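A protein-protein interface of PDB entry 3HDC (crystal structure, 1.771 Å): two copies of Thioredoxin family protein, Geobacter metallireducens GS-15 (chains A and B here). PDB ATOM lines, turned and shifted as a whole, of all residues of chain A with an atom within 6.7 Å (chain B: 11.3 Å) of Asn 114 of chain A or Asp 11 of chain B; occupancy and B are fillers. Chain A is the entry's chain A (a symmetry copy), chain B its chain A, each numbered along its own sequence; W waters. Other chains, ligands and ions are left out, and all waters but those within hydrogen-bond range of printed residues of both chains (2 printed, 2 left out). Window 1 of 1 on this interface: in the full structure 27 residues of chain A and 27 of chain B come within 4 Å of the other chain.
OD2 of Asp 11 of chain B is in hydrogen-bond range of NE2 of Gln 108 of chain A, at 2.9 Å. The backbone NH (N) of Leu 116 of chain A lies within hydrogen-bond range of the backbone carbonyl oxygen (O) of Glu 9 of chain B (2.8 Å). O of Ala 8 of chain B sits at hydrogen-bond distance from NH2 of Arg 115 of chain A (3.2 Å). N of Asp 11 of chain B lies within hydrogen-bond range of O of Asn 114 of chain A (2.8 Å).
The backbone NH of Ala 12 of chain B lies within hydrogen-bond range of the side-chain hydroxyl of Ser 10 of chain B (3.1 Å). NE2 of Gln 108 of chain A lies within hydrogen-bond range of O of Ala 113 of chain A (2.9 Å).
Among the printed residues, pairs that only touch across the chains: Trp 52 of chain A with Glu 9 of chain B, Trp 52 of chain A with Ser 10 of chain B, Trp 52 of chain A with Asp 11 of chain B, Val 82 of chain A with Asp 11 of chain B, Asn 114 of chain A with Ser 10 of chain B, Arg 115 of chain A with Glu 9 of chain B, Arg 115 of chain A with Ser 10 of chain B, Leu 116 of chain A with Ala 8 of chain B and Leu 116 of chain A with Asp 11 of chain B.
Of the printed residues of chain B, Trp 52 of chain A touches Glu 9, Ser 10 and Asp 11. Glu 83 of chain A touches none of the printed residues of chain B. Printed residues of chain B within 4 Å of Gln 108 of chain A: Asp 11 (2.9 Å). Tyr 111 of chain A touches none of the printed residues of chain B. Of chain B, only Ser 10 and Asp 11 come within 4 Å of Asn 114 of chain A. Leu 116 of chain A touches just these residues of chain B: Ala 8 (3.2 Å), Glu 9 (2.8 Å) and Asp 11 (3.7 Å). Of the printed residues of chain A, Ser 10 of chain B touches Trp 52, Asn 114 and Arg 115. Of chain A, only Trp 52 (3.4 Å), Val 82 (3.7 Å), Gln 108 (2.9 Å), Asn 114 (2.8 Å) and Leu 116 (3.7 Å) come within 4 Å of Asp 11 of chain B. The nearest residue of chain B that does not touch Asn 114 of chain A is Ala 12 of chain B (4.1 Å). The nearest residue of chain A that does not touch Asp 11 of chain B is Arg 115 of chain A (4.3 Å). The nearest printed residue of chain B that does not touch Gln 108 of chain A is Gln 109 of chain B (5.8 Å).
Printed residues of chain A that touch a printed residue of chain B: Trp 52, Val 82, Gln 108, Asn 114, Arg 115 and Leu 116. Along chain A the printed residues that touch a printed residue of chain B span positions 52 to 116. Of the 17 printed residues of chain B, 4 touch a printed residue of chain A. Among the printed residues, 13 pairs touch across the chains. Among the printed residues, no Asp or Glu carboxylate lies within 4 Å of a Lys or Arg side-chain nitrogen of the other chain.
Positions printed for both chains: 108, 111, 112, 113 and 114.
Water W2 bridges OG of Ser 10 of chain B and O of Asn 114 of chain A. Water W1 lies within hydrogen-bond range of O of Asp 11 of chain B (2.8 Å) and NE2 of Gln 108 of chain A (3.5 Å).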
ATOM      1  N   ALA A  50      18.904  -7.807  11.218  1.00  0.00           N
ATOM      2  CA  ALA A  50      19.155  -9.239  11.425  1.00  0.00           C
ATOM      3  C   ALA A  50      19.559  -9.469  12.873  1.00  0.00           C
ATOM      4  O   ALA A  50      20.255  -8.655  13.452  1.00  0.00           O
ATOM      5  CB  ALA A  50      20.255  -9.722  10.506  1.00  0.00           C
ATOM      6  N   TRP A  52      21.677 -11.408  14.123  1.00  0.00           N
ATOM      7  CA  TRP A  52      23.093 -11.679  14.331  1.00  0.00           C
ATOM      8  C   TRP A  52      23.935 -10.430  14.315  1.00  0.00           C
ATOM      9  O   TRP A  52      25.117 -10.480  14.642  1.00  0.00           O
ATOM     10  CB  TRP A  52      23.635 -12.692  13.301  1.00  0.00           C
ATOM     11  CG  TRP A  52      23.290 -12.383  11.861  1.00  0.00           C
ATOM     12  CD1 TRP A  52      22.329 -12.983  11.109  1.00  0.00           C
ATOM     13  CD2 TRP A  52      23.916 -11.414  11.012  1.00  0.00           C
ATOM     14  NE1 TRP A  52      22.312 -12.449   9.842  1.00  0.00           N
ATOM     15  CE2 TRP A  52      23.273 -11.484   9.753  1.00  0.00           C
ATOM     16  CE3 TRP A  52      24.951 -10.487  11.189  1.00  0.00           C
ATOM     17  CZ2 TRP A  52      23.633 -10.663   8.688  1.00  0.00           C
ATOM     18  CZ3 TRP A  52      25.310  -9.670  10.127  1.00  0.00           C
ATOM     19  CH2 TRP A  52      24.655  -9.765   8.884  1.00  0.00           C
ATOM     20  N   VAL A  82      15.572  -9.760   7.831  1.00  0.00           N
ATOM     21  CA  VAL A  82      16.051 -10.148   6.501  1.00  0.00           C
ATOM     22  C   VAL A  82      16.523 -11.597   6.443  1.00  0.00           C
ATOM     23  O   VAL A  82      16.979 -12.064   5.401  1.00  0.00           O
ATOM     24  CB  VAL A  82      17.210  -9.235   6.015  1.00  0.00           C
ATOM     25  CG1 VAL A  82      16.750  -7.770   5.921  1.00  0.00           C
ATOM     26  CG2 VAL A  82      18.434  -9.365   6.939  1.00  0.00           C
ATOM     27  N   GLU A  83      16.426 -12.299   7.564  1.00  0.00           N
ATOM     28  CA  GLU A  83      16.951 -13.664   7.660  1.00  0.00           C
ATOM     29  C   GLU A  83      16.015 -14.690   7.012  1.00  0.00           C
ATOM     30  O   GLU A  83      14.798 -14.494   6.941  1.00  0.00           O
ATOM     31  CB  GLU A  83      17.228 -14.044   9.121  1.00  0.00           C
ATOM     32  CG  GLU A  83      18.171 -13.108   9.839  1.00  0.00           C
ATOM     33  CD  GLU A  83      18.241 -13.400  11.316  1.00  0.00           C
ATOM     34  OE1 GLU A  83      17.645 -12.627  12.103  1.00  0.00           O
ATOM     35  OE2 GLU A  83      18.872 -14.417  11.693  1.00  0.00           O
ATOM     36  N   GLN A 108      13.984  -5.988   0.705  1.00  0.00           N
ATOM     37  CA  GLN A 108      15.308  -5.506   1.074  1.00  0.00           C
ATOM     38  C   GLN A 108      16.065  -5.051  -0.174  1.00  0.00           C
ATOM     39  O   GLN A 108      16.691  -3.993  -0.188  1.00  0.00           O
ATOM     40  CB  GLN A 108      16.099  -6.603   1.809  1.00  0.00           C
ATOM     41  CG  GLN A 108      17.469  -6.148   2.246  1.00  0.00           C
ATOM     42  CD  GLN A 108      18.318  -7.281   2.826  1.00  0.00           C
ATOM     43  OE1 GLN A 108      17.966  -8.459   2.720  1.00  0.00           O
ATOM     44  NE2 GLN A 108      19.442  -6.923   3.431  1.00  0.00           N
ATOM     45  N   TYR A 111      14.762  -1.737  -1.581  1.00  0.00           N
ATOM     46  CA  TYR A 111      15.243  -0.607  -0.792  1.00  0.00           C
ATOM     47  C   TYR A 111      16.756  -0.425  -0.847  1.00  0.00           C
ATOM     48  O   TYR A 111      17.273   0.536  -0.288  1.00  0.00           O
ATOM     49  CB  TYR A 111      14.773  -0.701   0.700  1.00  0.00           C
ATOM     50  CG  TYR A 111      13.395  -0.116   0.897  1.00  0.00           C
ATOM     51  CD1 TYR A 111      12.252  -0.825   0.504  1.00  0.00           C
ATOM     52  CD2 TYR A 111      13.236   1.167   1.422  1.00  0.00           C
ATOM     53  CE1 TYR A 111      10.976  -0.269   0.648  1.00  0.00           C
ATOM     54  CE2 TYR A 111      11.960   1.736   1.576  1.00  0.00           C
ATOM     55  CZ  TYR A 111      10.845   1.012   1.175  1.00  0.00           C
ATOM     56  OH  TYR A 111       9.589   1.551   1.305  1.00  0.00           O
ATOM     57  N   GLY A 112      17.461  -1.324  -1.536  1.00  0.00           N
ATOM     58  CA  GLY A 112      18.917  -1.262  -1.578  1.00  0.00           C
ATOM     59  C   GLY A 112      19.546  -1.346  -0.193  1.00  0.00           C
ATOM     60  O   GLY A 112      20.615  -0.776   0.064  1.00  0.00           O
ATOM     61  N   ALA A 113      18.892  -2.076   0.699  1.00  0.00           N
ATOM     62  CA  ALA A 113      19.302  -2.105   2.106  1.00  0.00           C
ATOM     63  C   ALA A 113      20.346  -3.195   2.328  1.00  0.00           C
ATOM     64  O   ALA A 113      20.078  -4.170   3.015  1.00  0.00           O
ATOM     65  CB  ALA A 113      18.109  -2.349   2.980  1.00  0.00           C
ATOM     66  N   ASN A 114      21.542  -2.992   1.789  1.00  0.00           N
ATOM     67  CA  ASN A 114      22.577  -4.032   1.838  1.00  0.00           C
ATOM     68  C   ASN A 114      23.561  -3.879   2.988  1.00  0.00           C
ATOM     69  O   ASN A 114      24.542  -4.598   3.037  1.00  0.00           O
ATOM     70  CB  ASN A 114      23.349  -4.118   0.512  1.00  0.00           C
ATOM     71  CG  ASN A 114      23.865  -2.782   0.042  1.00  0.00           C
ATOM     72  OD1 ASN A 114      24.267  -1.941   0.833  1.00  0.00           O
ATOM     73  ND2 ASN A 114      23.855  -2.573  -1.282  1.00  0.00           N
ATOM     74  N   ARG A 115      23.305  -2.941   3.901  1.00  0.00           N
ATOM     75  CA  ARG A 115      24.059  -2.843   5.150  1.00  0.00           C
ATOM     76  C   ARG A 115      23.014  -2.727   6.251  1.00  0.00           C
ATOM     77  O   ARG A 115      21.969  -2.111   6.038  1.00  0.00           O
ATOM     78  CB  ARG A 115      24.961  -1.606   5.152  1.00  0.00           C
ATOM     79  CG  ARG A 115      26.108  -1.687   4.125  1.00  0.00           C
ATOM     80  CD  ARG A 115      27.056  -0.500   4.214  1.00  0.00           C
ATOM     81  NE  ARG A 115      27.860  -0.530   5.433  1.00  0.00           N
ATOM     82  CZ  ARG A 115      28.883  -1.356   5.654  1.00  0.00           C
ATOM     83  NH1 ARG A 115      29.259  -2.241   4.732  1.00  0.00           N
ATOM     84  NH2 ARG A 115      29.539  -1.293   6.802  1.00  0.00           N
ATOM     85  N   LEU A 116      23.283  -3.309   7.413  1.00  0.00           N
ATOM     86  CA  LEU A 116      22.281  -3.397   8.476  1.00  0.00           C
ATOM     87  C   LEU A 116      22.849  -2.859   9.780  1.00  0.00           C
ATOM     88  O   LEU A 116      24.027  -3.008  10.045  1.00  0.00           O
ATOM     89  CB  LEU A 116      21.925  -4.865   8.729  1.00  0.00           C
ATOM     90  CG  LEU A 116      21.453  -5.652   7.506  1.00  0.00           C
ATOM     91  CD1 LEU A 116      21.271  -7.117   7.914  1.00  0.00           C
ATOM     92  CD2 LEU A 116      20.170  -5.071   7.035  1.00  0.00           C
ATOM     93  N   ASP A 118      19.414  -0.727   8.556  1.00  0.00           N
ATOM     94  CA  ASP A 118      19.199   0.341   7.590  1.00  0.00           C
ATOM     95  C   ASP A 118      17.764   0.782   7.815  1.00  0.00           C
ATOM     96  O   ASP A 118      16.841  -0.037   7.752  1.00  0.00           O
ATOM     97  CB  ASP A 118      19.380  -0.206   6.175  1.00  0.00           C
ATOM     98  CG  ASP A 118      19.830   0.838   5.193  1.00  0.00           C
ATOM     99  OD1 ASP A 118      20.195   1.959   5.598  1.00  0.00           O
ATOM    100  OD2 ASP A 118      19.832   0.521   3.982  1.00  0.00           O
ATOM    101  N   LYS B   7      27.183   2.674  13.216  1.00  0.00           N
ATOM    102  CA  LYS B   7      27.896   1.498  12.720  1.00  0.00           C
ATOM    103  C   LYS B   7      26.924   0.508  12.083  1.00  0.00           C
ATOM    104  O   LYS B   7      25.812   0.306  12.577  1.00  0.00           O
ATOM    105  CB  LYS B   7      28.668   0.821  13.861  1.00  0.00           C
ATOM    106  CG  LYS B   7      29.776   1.687  14.428  1.00  0.00           C
ATOM    107  CD  LYS B   7      30.470   0.978  15.585  1.00  0.00           C
ATOM    108  CE  LYS B   7      31.615   1.817  16.142  1.00  0.00           C
ATOM    109  NZ  LYS B   7      32.263   1.166  17.321  1.00  0.00           N
ATOM    110  N   ALA B   8      27.353  -0.105  10.982  1.00  0.00           N
ATOM    111  CA  ALA B   8      26.531  -1.050  10.241  1.00  0.00           C
ATOM    112  C   ALA B   8      27.419  -2.201   9.793  1.00  0.00           C
ATOM    113  O   ALA B   8      28.642  -2.052   9.748  1.00  0.00           O
ATOM    114  CB  ALA B   8      25.914  -0.369   9.017  1.00  0.00           C
ATOM    115  N   GLU B   9      26.812  -3.341   9.473  1.00  0.00           N
ATOM    116  CA  GLU B   9      27.554  -4.441   8.852  1.00  0.00           C
ATOM    117  C   GLU B   9      26.967  -4.805   7.491  1.00  0.00           C
ATOM    118  O   GLU B   9      25.777  -4.668   7.261  1.00  0.00           O
ATOM    119  CB  GLU B   9      27.576  -5.667   9.758  1.00  0.00           C
ATOM    120  CG  GLU B   9      28.270  -5.383  11.094  1.00  0.00           C
ATOM    121  CD  GLU B   9      28.520  -6.628  11.929  1.00  0.00           C
ATOM    122  OE1 GLU B   9      27.711  -7.570  11.896  1.00  0.00           O
ATOM    123  OE2 GLU B   9      29.530  -6.636  12.651  1.00  0.00           O
ATOM    124  N   SER B  10      27.813  -5.286   6.592  1.00  0.00           N
ATOM    125  CA  SER B  10      27.328  -5.700   5.271  1.00  0.00           C
ATOM    126  C   SER B  10      26.384  -6.884   5.349  1.00  0.00           C
ATOM    127  O   SER B  10      26.623  -7.814   6.121  1.00  0.00           O
ATOM    128  CB  SER B  10      28.519  -6.076   4.381  1.00  0.00           C
ATOM    129  OG  SER B  10      28.084  -6.482   3.095  1.00  0.00           O
ATOM    130  N   ASP B  11      25.330  -6.877   4.524  1.00  0.00           N
ATOM    131  CA  ASP B  11      24.501  -8.056   4.355  1.00  0.00           C
ATOM    132  C   ASP B  11      24.636  -8.662   2.962  1.00  0.00           C
ATOM    133  O   ASP B  11      23.707  -9.275   2.457  1.00  0.00           O
ATOM    134  CB  ASP B  11      23.041  -7.775   4.672  1.00  0.00           C
ATOM    135  CG  ASP B  11      22.230  -9.036   4.843  1.00  0.00           C
ATOM    136  OD1 ASP B  11      22.750 -10.011   5.442  1.00  0.00           O
ATOM    137  OD2 ASP B  11      21.064  -9.064   4.402  1.00  0.00           O
ATOM    138  N   ALA B  12      25.802  -8.488   2.356  1.00  0.00           N
ATOM    139  CA  ALA B  12      26.062  -9.085   1.042  1.00  0.00           C
ATOM    140  C   ALA B  12      27.188 -10.102   1.154  1.00  0.00           C
ATOM    141  O   ALA B  12      28.140  -9.866   1.875  1.00  0.00           O
ATOM    142  CB  ALA B  12      26.460  -8.009   0.076  1.00  0.00           C
ATOM    143  N   PRO B  13      27.080 -11.226   0.428  1.00  0.00           N
ATOM    144  CA  PRO B  13      28.242 -12.121   0.351  1.00  0.00           C
ATOM    145  C   PRO B  13      29.317 -11.449  -0.490  1.00  0.00           C
ATOM    146  O   PRO B  13      29.060 -10.403  -1.092  1.00  0.00           O
ATOM    147  CB  PRO B  13      27.702 -13.370  -0.347  1.00  0.00           C
ATOM    148  CG  PRO B  13      26.460 -12.936  -1.076  1.00  0.00           C
ATOM    149  CD  PRO B  13      25.969 -11.637  -0.446  1.00  0.00           C
ATOM    150  N   LEU B  14      30.507 -12.035  -0.547  1.00  0.00           N
ATOM    151  CA  LEU B  14      31.642 -11.348  -1.136  1.00  0.00           C
ATOM    152  C   LEU B  14      31.855 -11.718  -2.587  1.00  0.00           C
ATOM    153  O   LEU B  14      31.638 -12.857  -2.984  1.00  0.00           O
ATOM    154  CB  LEU B  14      32.925 -11.702  -0.371  1.00  0.00           C
ATOM    155  CG  LEU B  14      32.850 -11.489   1.128  1.00  0.00           C
ATOM    156  CD1 LEU B  14      34.151 -11.996   1.782  1.00  0.00           C
ATOM    157  CD2 LEU B  14      32.591 -10.005   1.420  1.00  0.00           C
ATOM    158  N   VAL B  15      32.303 -10.749  -3.375  1.00  0.00           N
ATOM    159  CA  VAL B  15      32.720 -11.032  -4.751  1.00  0.00           C
ATOM    160  C   VAL B  15      33.934 -10.137  -4.999  1.00  0.00           C
ATOM    161  O   VAL B  15      33.857  -8.914  -4.869  1.00  0.00           O
ATOM    162  CB  VAL B  15      31.571 -10.830  -5.775  1.00  0.00           C
ATOM    163  CG1 VAL B  15      30.860  -9.504  -5.563  1.00  0.00           C
ATOM    164  CG2 VAL B  15      32.106 -10.911  -7.210  1.00  0.00           C
ATOM    165  N   GLN B 106      19.065 -14.724  -7.525  1.00  0.00           N
ATOM    166  CA  GLN B 106      20.087 -14.962  -6.521  1.00  0.00           C
ATOM    167  C   GLN B 106      21.492 -14.859  -7.072  1.00  0.00           C
ATOM    168  O   GLN B 106      22.372 -14.352  -6.411  1.00  0.00           O
ATOM    169  CB  GLN B 106      19.911 -16.342  -5.872  1.00  0.00           C
ATOM    170  CG  GLN B 106      18.625 -16.483  -5.059  1.00  0.00           C
ATOM    171  CD  GLN B 106      18.548 -15.492  -3.930  1.00  0.00           C
ATOM    172  OE1 GLN B 106      17.968 -14.411  -4.074  1.00  0.00           O
ATOM    173  NE2 GLN B 106      19.138 -15.847  -2.787  1.00  0.00           N
ATOM    174  N   GLN B 108      22.657 -13.221  -9.711  1.00  0.00           N
ATOM    175  CA  GLN B 108      22.950 -11.831 -10.032  1.00  0.00           C
ATOM    176  C   GLN B 108      23.260 -11.053  -8.753  1.00  0.00           C
ATOM    177  O   GLN B 108      24.215 -10.281  -8.693  1.00  0.00           O
ATOM    178  CB  GLN B 108      21.769 -11.186 -10.778  1.00  0.00           C
ATOM    179  CG  GLN B 108      22.031  -9.752 -11.168  1.00  0.00           C
ATOM    180  CD  GLN B 108      20.802  -9.060 -11.759  1.00  0.00           C
ATOM    181  OE1 GLN B 108      19.685  -9.581 -11.696  1.00  0.00           O
ATOM    182  NE2 GLN B 108      21.008  -7.879 -12.326  1.00  0.00           N
ATOM    183  N   GLN B 109      22.471 -11.292  -7.719  1.00  0.00           N
ATOM    184  CA  GLN B 109      22.684 -10.604  -6.445  1.00  0.00           C
ATOM    185  C   GLN B 109      24.021 -10.993  -5.803  1.00  0.00           C
ATOM    186  O   GLN B 109      24.757 -10.144  -5.305  1.00  0.00           O
ATOM    187  CB  GLN B 109      21.505 -10.891  -5.498  1.00  0.00           C
ATOM    188  CG  GLN B 109      21.591 -10.169  -4.159  1.00  0.00           C
ATOM    189  CD  GLN B 109      20.251 -10.132  -3.451  1.00  0.00           C
ATOM    190  OE1 GLN B 109      19.413 -11.022  -3.635  1.00  0.00           O
ATOM    191  NE2 GLN B 109      20.027  -9.093  -2.664  1.00  0.00           N
ATOM    192  N   ARG B 110      24.355 -12.280  -5.842  1.00  0.00           N
ATOM    193  CA  ARG B 110      25.608 -12.731  -5.265  1.00  0.00           C
ATOM    194  C   ARG B 110      26.821 -12.160  -5.981  1.00  0.00           C
ATOM    195  O   ARG B 110      27.865 -11.954  -5.360  1.00  0.00           O
ATOM    196  CB  ARG B 110      25.665 -14.256  -5.231  1.00  0.00           C
ATOM    197  CG  ARG B 110      24.610 -14.847  -4.283  1.00  0.00           C
ATOM    198  CD  ARG B 110      24.454 -16.333  -4.523  1.00  0.00           C
ATOM    199  NE  ARG B 110      25.732 -16.976  -4.294  1.00  0.00           N
ATOM    200  CZ  ARG B 110      26.172 -18.042  -4.946  1.00  0.00           C
ATOM    201  NH1 ARG B 110      25.411 -18.630  -5.880  1.00  0.00           N
ATOM    202  NH2 ARG B 110      27.383 -18.524  -4.630  1.00  0.00           N
ATOM    203  N   TYR B 111      26.691 -11.903  -7.284  1.00  0.00           N
ATOM    204  CA  TYR B 111      27.759 -11.242  -8.028  1.00  0.00           C
ATOM    205  C   TYR B 111      27.718  -9.721  -7.930  1.00  0.00           C
ATOM    206  O   TYR B 111      28.607  -9.055  -8.448  1.00  0.00           O
ATOM    207  CB  TYR B 111      27.771 -11.677  -9.533  1.00  0.00           C
ATOM    208  CG  TYR B 111      28.555 -12.949  -9.747  1.00  0.00           C
ATOM    209  CD1 TYR B 111      28.010 -14.195  -9.403  1.00  0.00           C
ATOM    210  CD2 TYR B 111      29.860 -12.907 -10.239  1.00  0.00           C
ATOM    211  CE1 TYR B 111      28.749 -15.371  -9.564  1.00  0.00           C
ATOM    212  CE2 TYR B 111      30.612 -14.082 -10.408  1.00  0.00           C
ATOM    213  CZ  TYR B 111      30.047 -15.301 -10.056  1.00  0.00           C
ATOM    214  OH  TYR B 111      30.767 -16.462 -10.202  1.00  0.00           O
ATOM    215  N   GLY B 112      26.709  -9.172  -7.249  1.00  0.00           N
ATOM    216  CA  GLY B 112      26.558  -7.725  -7.169  1.00  0.00           C
ATOM    217  C   GLY B 112      26.418  -7.075  -8.540  1.00  0.00           C
ATOM    218  O   GLY B 112      26.834  -5.928  -8.754  1.00  0.00           O
ATOM    219  N   ALA B 113      25.813  -7.801  -9.469  1.00  0.00           N
ATOM    220  CA  ALA B 113      25.761  -7.360 -10.865  1.00  0.00           C
ATOM    221  C   ALA B 113      24.536  -6.478 -11.093  1.00  0.00           C
ATOM    222  O   ALA B 113      23.628  -6.864 -11.814  1.00  0.00           O
ATOM    223  CB  ALA B 113      25.714  -8.550 -11.775  1.00  0.00           C
ATOM    224  N   ASN B 114      24.550  -5.282 -10.518  1.00  0.00           N
ATOM    225  CA  ASN B 114      23.372  -4.406 -10.572  1.00  0.00           C
ATOM    226  C   ASN B 114      23.410  -3.378 -11.692  1.00  0.00           C
ATOM    227  O   ASN B 114      22.558  -2.510 -11.737  1.00  0.00           O
ATOM    228  CB  ASN B 114      23.142  -3.693  -9.229  1.00  0.00           C
ATOM    229  CG  ASN B 114      24.377  -3.003  -8.709  1.00  0.00           C
ATOM    230  OD1 ASN B 114      25.171  -2.462  -9.465  1.00  0.00           O
ATOM    231  ND2 ASN B 114      24.552  -3.022  -7.380  1.00  0.00           N
HETATM  232  O   HOH W   1      21.361  -8.604   1.108  1.00  0.00           O
HETATM  233  O   HOH W   2      26.999  -4.493   1.486  1.00  0.00           O
